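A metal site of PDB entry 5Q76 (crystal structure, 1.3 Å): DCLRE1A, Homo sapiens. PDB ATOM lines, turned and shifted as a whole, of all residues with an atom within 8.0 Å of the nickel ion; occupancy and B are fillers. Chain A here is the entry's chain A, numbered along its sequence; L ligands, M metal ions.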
ATOM      1  N   ASP A  18     -20.660  -8.092  18.577  1.00  0.00           N
ATOM      2  CA  ASP A  18     -19.518  -8.449  19.476  1.00  0.00           C
ATOM      3  C   ASP A  18     -18.989  -9.911  19.238  1.00  0.00           C
ATOM      4  O   ASP A  18     -18.783 -10.684  20.209  1.00  0.00           O
ATOM      5  CB  ASP A  18     -19.857  -8.157  20.909  1.00  0.00           C
ATOM      6  CG  ASP A  18     -20.224  -6.635  21.171  1.00  0.00           C
ATOM      7  OD1 ASP A  18     -19.952  -5.799  20.288  1.00  0.00           O
ATOM      8  OD2 ASP A  18     -20.715  -6.397  22.298  1.00  0.00           O
ATOM      9  N   THR A  34     -20.200  -3.017  19.981  1.00  0.00           N
ATOM     10  CA  THR A  34     -20.875  -2.091  20.924  1.00  0.00           C
ATOM     11  C   THR A  34     -19.920  -1.145  21.668  1.00  0.00           C
ATOM     12  O   THR A  34     -20.274   0.012  21.899  1.00  0.00           O
ATOM     13  CB  THR A  34     -21.749  -2.847  21.922  1.00  0.00           C
ATOM     14  OG1 THR A  34     -20.949  -3.692  22.800  1.00  0.00           O
ATOM     15  CG2 THR A  34     -22.860  -3.679  21.271  1.00  0.00           C
ATOM     16  N   HIS A  35     -18.727  -1.633  22.016  1.00  0.00           N
ATOM     17  CA  HIS A  35     -17.752  -0.845  22.805  1.00  0.00           C
ATOM     18  C   HIS A  35     -16.386  -1.495  22.788  1.00  0.00           C
ATOM     19  O   HIS A  35     -16.263  -2.728  22.548  1.00  0.00           O
ATOM     20  CB  HIS A  35     -18.312  -0.587  24.247  1.00  0.00           C
ATOM     21  CG  HIS A  35     -18.399  -1.765  25.161  1.00  0.00           C
ATOM     22  ND1 HIS A  35     -19.269  -2.845  25.006  1.00  0.00           N
ATOM     23  CD2 HIS A  35     -17.684  -2.048  26.287  1.00  0.00           C
ATOM     24  CE1 HIS A  35     -19.094  -3.666  26.042  1.00  0.00           C
ATOM     25  NE2 HIS A  35     -18.174  -3.166  26.823  1.00  0.00           N
ATOM     26  N   PHE A  36     -15.429  -0.683  23.146  1.00  0.00           N
ATOM     27  CA  PHE A  36     -13.987  -1.113  23.159  1.00  0.00           C
ATOM     28  C   PHE A  36     -13.548  -1.758  24.491  1.00  0.00           C
ATOM     29  O   PHE A  36     -12.705  -1.122  25.206  1.00  0.00           O
ATOM     30  CB  PHE A  36     -13.042   0.054  22.723  1.00  0.00           C
ATOM     31  CG  PHE A  36     -11.650  -0.356  22.338  1.00  0.00           C
ATOM     32  CD1 PHE A  36     -11.433  -0.922  21.096  1.00  0.00           C
ATOM     33  CD2 PHE A  36     -10.577  -0.142  23.199  1.00  0.00           C
ATOM     34  CE1 PHE A  36     -10.117  -1.305  20.737  1.00  0.00           C
ATOM     35  CE2 PHE A  36      -9.266  -0.516  22.840  1.00  0.00           C
ATOM     36  CZ  PHE A  36      -9.029  -1.058  21.618  1.00  0.00           C
ATOM     37  N   HIS A  37     -14.098  -2.911  24.871  1.00  0.00           N
ATOM     38  CA  HIS A  37     -13.649  -3.751  26.012  1.00  0.00           C
ATOM     39  C   HIS A  37     -13.243  -5.139  25.416  1.00  0.00           C
ATOM     40  O   HIS A  37     -13.885  -5.666  24.484  1.00  0.00           O
ATOM     41  CB  HIS A  37     -14.709  -3.937  27.093  1.00  0.00           C
ATOM     42  CG  HIS A  37     -14.826  -2.779  28.070  1.00  0.00           C
ATOM     43  ND1 HIS A  37     -15.899  -2.598  28.933  1.00  0.00           N
ATOM     44  CD2 HIS A  37     -13.966  -1.778  28.324  1.00  0.00           C
ATOM     45  CE1 HIS A  37     -15.670  -1.547  29.705  1.00  0.00           C
ATOM     46  NE2 HIS A  37     -14.515  -1.017  29.325  1.00  0.00           N
ATOM     47  N   SER A  38     -12.164  -5.732  25.986  1.00  0.00           N
ATOM     48  CA  SER A  38     -11.477  -6.860  25.326  1.00  0.00           C
ATOM     49  C   SER A  38     -12.369  -8.064  25.219  1.00  0.00           C
ATOM     50  O   SER A  38     -12.267  -8.773  24.177  1.00  0.00           O
ATOM     51  CB  SER A  38     -10.080  -7.081  25.943  1.00  0.00           C
ATOM     52  OG  SER A  38     -10.232  -7.370  27.307  1.00  0.00           O
ATOM     53  N   ASP A  39     -13.231  -8.367  26.164  1.00  0.00           N
ATOM     54  CA  ASP A  39     -14.149  -9.566  26.031  1.00  0.00           C
ATOM     55  C   ASP A  39     -15.053  -9.390  24.784  1.00  0.00           C
ATOM     56  O   ASP A  39     -15.545 -10.403  24.210  1.00  0.00           O
ATOM     57  CB  ASP A  39     -14.993  -9.823  27.270  1.00  0.00           C
ATOM     58  CG  ASP A  39     -14.233 -10.599  28.421  1.00  0.00           C
ATOM     59  OD1 ASP A  39     -13.052 -10.939  28.253  1.00  0.00           O
ATOM     60  OD2 ASP A  39     -14.928 -10.798  29.461  1.00  0.00           O
ATOM     61  N   HIS A  40     -15.303  -8.133  24.370  1.00  0.00           N
ATOM     62  CA  HIS A  40     -16.180  -7.831  23.201  1.00  0.00           C
ATOM     63  C   HIS A  40     -15.479  -7.673  21.901  1.00  0.00           C
ATOM     64  O   HIS A  40     -16.006  -8.132  20.843  1.00  0.00           O
ATOM     65  CB  HIS A  40     -17.030  -6.580  23.556  1.00  0.00           C
ATOM     66  CG  HIS A  40     -17.880  -6.788  24.731  1.00  0.00           C
ATOM     67  ND1 HIS A  40     -19.224  -7.068  24.676  1.00  0.00           N
ATOM     68  CD2 HIS A  40     -17.572  -6.815  26.052  1.00  0.00           C
ATOM     69  CE1 HIS A  40     -19.702  -7.268  25.877  1.00  0.00           C
ATOM     70  NE2 HIS A  40     -18.694  -7.139  26.736  1.00  0.00           N
ATOM     71  N   HIS A  96     -22.197   3.467  29.594  1.00  0.00           N
ATOM     72  CA  HIS A  96     -21.168   2.465  30.046  1.00  0.00           C
ATOM     73  C   HIS A  96     -19.822   3.155  29.998  1.00  0.00           C
ATOM     74  O   HIS A  96     -19.697   4.137  30.807  1.00  0.00           O
ATOM     75  CB  HIS A  96     -21.278   1.199  29.197  1.00  0.00           C
ATOM     76  CG  HIS A  96     -20.380   0.019  29.518  1.00  0.00           C
ATOM     77  ND1 HIS A  96     -20.287  -0.484  30.788  1.00  0.00           N
ATOM     78  CD2 HIS A  96     -19.476  -0.679  28.771  1.00  0.00           C
ATOM     79  CE1 HIS A  96     -19.436  -1.508  30.804  1.00  0.00           C
ATOM     80  NE2 HIS A  96     -18.919  -1.656  29.593  1.00  0.00           N
ATOM     81  N   CYS A  97     -18.869   2.780  29.176  1.00  0.00           N
ATOM     82  CA  CYS A  97     -17.556   3.496  28.970  1.00  0.00           C
ATOM     83  C   CYS A  97     -17.672   4.442  27.778  1.00  0.00           C
ATOM     84  O   CYS A  97     -18.632   4.371  27.018  1.00  0.00           O
ATOM     85  CB  CYS A  97     -16.435   2.439  28.807  1.00  0.00           C
ATOM     86  SG  CYS A  97     -16.631   1.404  27.292  1.00  0.00           S
ATOM     87  N   ALA A 100     -19.464   3.643  24.111  1.00  0.00           N
ATOM     88  CA  ALA A 100     -20.356   2.446  24.238  1.00  0.00           C
ATOM     89  C   ALA A 100     -21.774   2.796  23.788  1.00  0.00           C
ATOM     90  O   ALA A 100     -22.307   3.839  24.166  1.00  0.00           O
ATOM     91  CB  ALA A 100     -20.351   1.892  25.633  1.00  0.00           C
ATOM     92  N   GLY A 117     -25.813  -3.987  24.427  1.00  0.00           N
ATOM     93  CA  GLY A 117     -24.382  -4.158  24.711  1.00  0.00           C
ATOM     94  C   GLY A 117     -24.198  -4.219  26.207  1.00  0.00           C
ATOM     95  O   GLY A 117     -25.006  -4.813  26.887  1.00  0.00           O
ATOM     96  N   ASP A 118     -23.111  -3.632  26.723  1.00  0.00           N
ATOM     97  CA  ASP A 118     -22.998  -3.390  28.184  1.00  0.00           C
ATOM     98  C   ASP A 118     -23.620  -2.000  28.480  1.00  0.00           C
ATOM     99  O   ASP A 118     -23.368  -1.003  27.723  1.00  0.00           O
ATOM    100  CB  ASP A 118     -21.570  -3.388  28.618  1.00  0.00           C
ATOM    101  CG  ASP A 118     -20.923  -4.819  28.777  1.00  0.00           C
ATOM    102  OD1 ASP A 118     -21.687  -5.796  28.714  1.00  0.00           O
ATOM    103  OD2 ASP A 118     -19.708  -4.865  28.996  1.00  0.00           O
ATOM    104  N   PHE A 119     -24.416  -1.897  29.549  1.00  0.00           N
ATOM    105  CA  PHE A 119     -25.091  -0.607  29.853  1.00  0.00           C
ATOM    106  C   PHE A 119     -25.327  -0.412  31.344  1.00  0.00           C
ATOM    107  O   PHE A 119     -25.367  -1.367  32.113  1.00  0.00           O
ATOM    108  CB  PHE A 119     -26.399  -0.374  29.034  1.00  0.00           C
ATOM    109  CG  PHE A 119     -27.734  -0.971  29.560  1.00  0.00           C
ATOM    110  CD1 PHE A 119     -28.924  -0.229  29.479  1.00  0.00           C
ATOM    111  CD2 PHE A 119     -27.797  -2.305  30.109  1.00  0.00           C
ATOM    112  CE1 PHE A 119     -30.141  -0.770  29.870  1.00  0.00           C
ATOM    113  CE2 PHE A 119     -29.018  -2.808  30.567  1.00  0.00           C
ATOM    114  CZ  PHE A 119     -30.170  -2.051  30.396  1.00  0.00           C
ATOM    115  N   ASP A 141     -27.931  -6.850  28.937  1.00  0.00           N
ATOM    116  CA  ASP A 141     -26.743  -6.948  29.843  1.00  0.00           C
ATOM    117  C   ASP A 141     -27.294  -7.218  31.266  1.00  0.00           C
ATOM    118  O   ASP A 141     -27.801  -6.365  31.974  1.00  0.00           O
ATOM    119  CB  ASP A 141     -25.930  -5.648  29.831  1.00  0.00           C
ATOM    120  CG  ASP A 141     -24.892  -5.560  30.960  1.00  0.00           C
ATOM    121  OD1 ASP A 141     -24.598  -6.612  31.589  1.00  0.00           O
ATOM    122  OD2 ASP A 141     -24.408  -4.397  31.166  1.00  0.00           O
ATOM    123  N   THR A 143     -25.406  -8.489  33.839  1.00  0.00           N
ATOM    124  CA  THR A 143     -24.271  -8.689  34.722  1.00  0.00           C
ATOM    125  C   THR A 143     -24.670  -8.732  36.161  1.00  0.00           C
ATOM    126  O   THR A 143     -24.279  -9.706  36.913  1.00  0.00           O
ATOM    127  CB  THR A 143     -23.253  -7.496  34.515  1.00  0.00           C
ATOM    128  OG1 THR A 143     -22.677  -7.503  33.197  1.00  0.00           O
ATOM    129  CG2 THR A 143     -22.060  -7.654  35.499  1.00  0.00           C
ATOM    130  N   SER A 183      -8.536  -0.782  31.567  1.00  0.00           N
ATOM    131  CA  SER A 183      -9.450  -0.721  30.406  1.00  0.00           C
ATOM    132  C   SER A 183      -9.957   0.731  30.372  1.00  0.00           C
ATOM    133  O   SER A 183      -9.864   1.470  31.393  1.00  0.00           O
ATOM    134  CB  SER A 183     -10.701  -1.639  30.527  1.00  0.00           C
ATOM    135  OG  SER A 183     -11.481  -1.323  31.677  1.00  0.00           O
ATOM    136  N   ILE A 184     -10.586   1.137  29.287  1.00  0.00           N
ATOM    137  CA  ILE A 184     -11.298   2.403  29.275  1.00  0.00           C
ATOM    138  C   ILE A 184     -12.535   2.283  30.146  1.00  0.00           C
ATOM    139  O   ILE A 184     -13.009   1.158  30.485  1.00  0.00           O
ATOM    140  CB  ILE A 184     -11.700   2.852  27.843  1.00  0.00           C
ATOM    141  CG1 ILE A 184     -12.739   1.967  27.151  1.00  0.00           C
ATOM    142  CG2 ILE A 184     -10.427   3.022  27.035  1.00  0.00           C
ATOM    143  CD1 ILE A 184     -13.356   2.576  25.925  1.00  0.00           C
ATOM    144  N   GLU A 296     -20.145   0.809  36.118  1.00  0.00           N
ATOM    145  CA  GLU A 296     -20.669   1.170  34.744  1.00  0.00           C
ATOM    146  C   GLU A 296     -21.677   0.104  34.176  1.00  0.00           C
ATOM    147  O   GLU A 296     -21.954   0.043  32.985  1.00  0.00           O
ATOM    148  CB  GLU A 296     -19.543   1.518  33.763  1.00  0.00           C
ATOM    149  CG  GLU A 296     -18.851   2.864  34.173  1.00  0.00           C
ATOM    150  CD  GLU A 296     -17.799   3.341  33.182  1.00  0.00           C
ATOM    151  OE1 GLU A 296     -17.229   2.586  32.377  1.00  0.00           O
ATOM    152  OE2 GLU A 296     -17.475   4.590  33.296  1.00  0.00           O
ATOM    153  N   HIS A 297     -22.207  -0.738  35.104  1.00  0.00           N
ATOM    154  CA  HIS A 297     -23.324  -1.639  34.773  1.00  0.00           C
ATOM    155  C   HIS A 297     -24.537  -1.340  35.659  1.00  0.00           C
ATOM    156  O   HIS A 297     -24.399  -0.865  36.818  1.00  0.00           O
ATOM    157  CB  HIS A 297     -22.947  -3.141  34.976  1.00  0.00           C
ATOM    158  CG  HIS A 297     -21.898  -3.640  34.082  1.00  0.00           C
ATOM    159  ND1 HIS A 297     -22.148  -4.187  32.824  1.00  0.00           N
ATOM    160  CD2 HIS A 297     -20.553  -3.820  34.296  1.00  0.00           C
ATOM    161  CE1 HIS A 297     -21.006  -4.568  32.291  1.00  0.00           C
ATOM    162  NE2 HIS A 297     -20.043  -4.371  33.157  1.00  0.00           N
HETATM  163  C1  LIG L   1     -15.966  -5.575  31.047  1.00  0.00           C
HETATM  164  C2  LIG L   1     -17.058  -4.847  31.789  1.00  0.00           C
HETATM  165  C3  LIG L   1     -16.440  -6.177  29.709  1.00  0.00           C
HETATM  166  O1  LIG L   1     -17.330  -5.034  32.980  1.00  0.00           O
HETATM  167  O2  LIG L   1     -17.706  -4.010  31.169  1.00  0.00           O
HETATM  168  O3  LIG L   1     -16.994  -5.468  28.836  1.00  0.00           O
HETATM  169  O4  LIG L   1     -16.171  -7.383  29.472  1.00  0.00           O
HETATM  170 NI    NI M   1     -17.894  -3.635  29.016  1.00  0.00          NI
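Within 4 Å of the nickel ion: His 35, His 37, His 96 and Asp 118.
The nearest printed residue that does not touch the nickel ion is His 40 (4.3 Å).
The nickel ion is bound by O3 of the ligand (2.0 Å).
The side-chain carboxylate (OD2) of Asp 118 is bound to the nickel ion (2.2 Å).
O2 of the ligand binds the nickel ion (2.2 Å).
ND1 of His 37 is bound to the nickel ion (2.2 Å).
NE2 of His 35 binds the nickel ion, 2.3 Å away.
The nickel ion is bound by NE2 of His 96, 2.3 Å away.
The nickel ion has six donor atoms within binding distance.
NE2 of His 40 sits close to OD2 of Asp 118 (3.4 Å).
A ring nitrogen (NE2) of His 37 is in hydrogen-bond range of the backbone carbonyl oxygen (O) of Ile 184 (2.9 Å).
ND1 of His 35 lies within hydrogen-bond range of OG1 of Thr 34, at 2.9 Å.
ND1 of His 96 sits at hydrogen-bond distance from O of Glu 296, at 2.8 Å.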
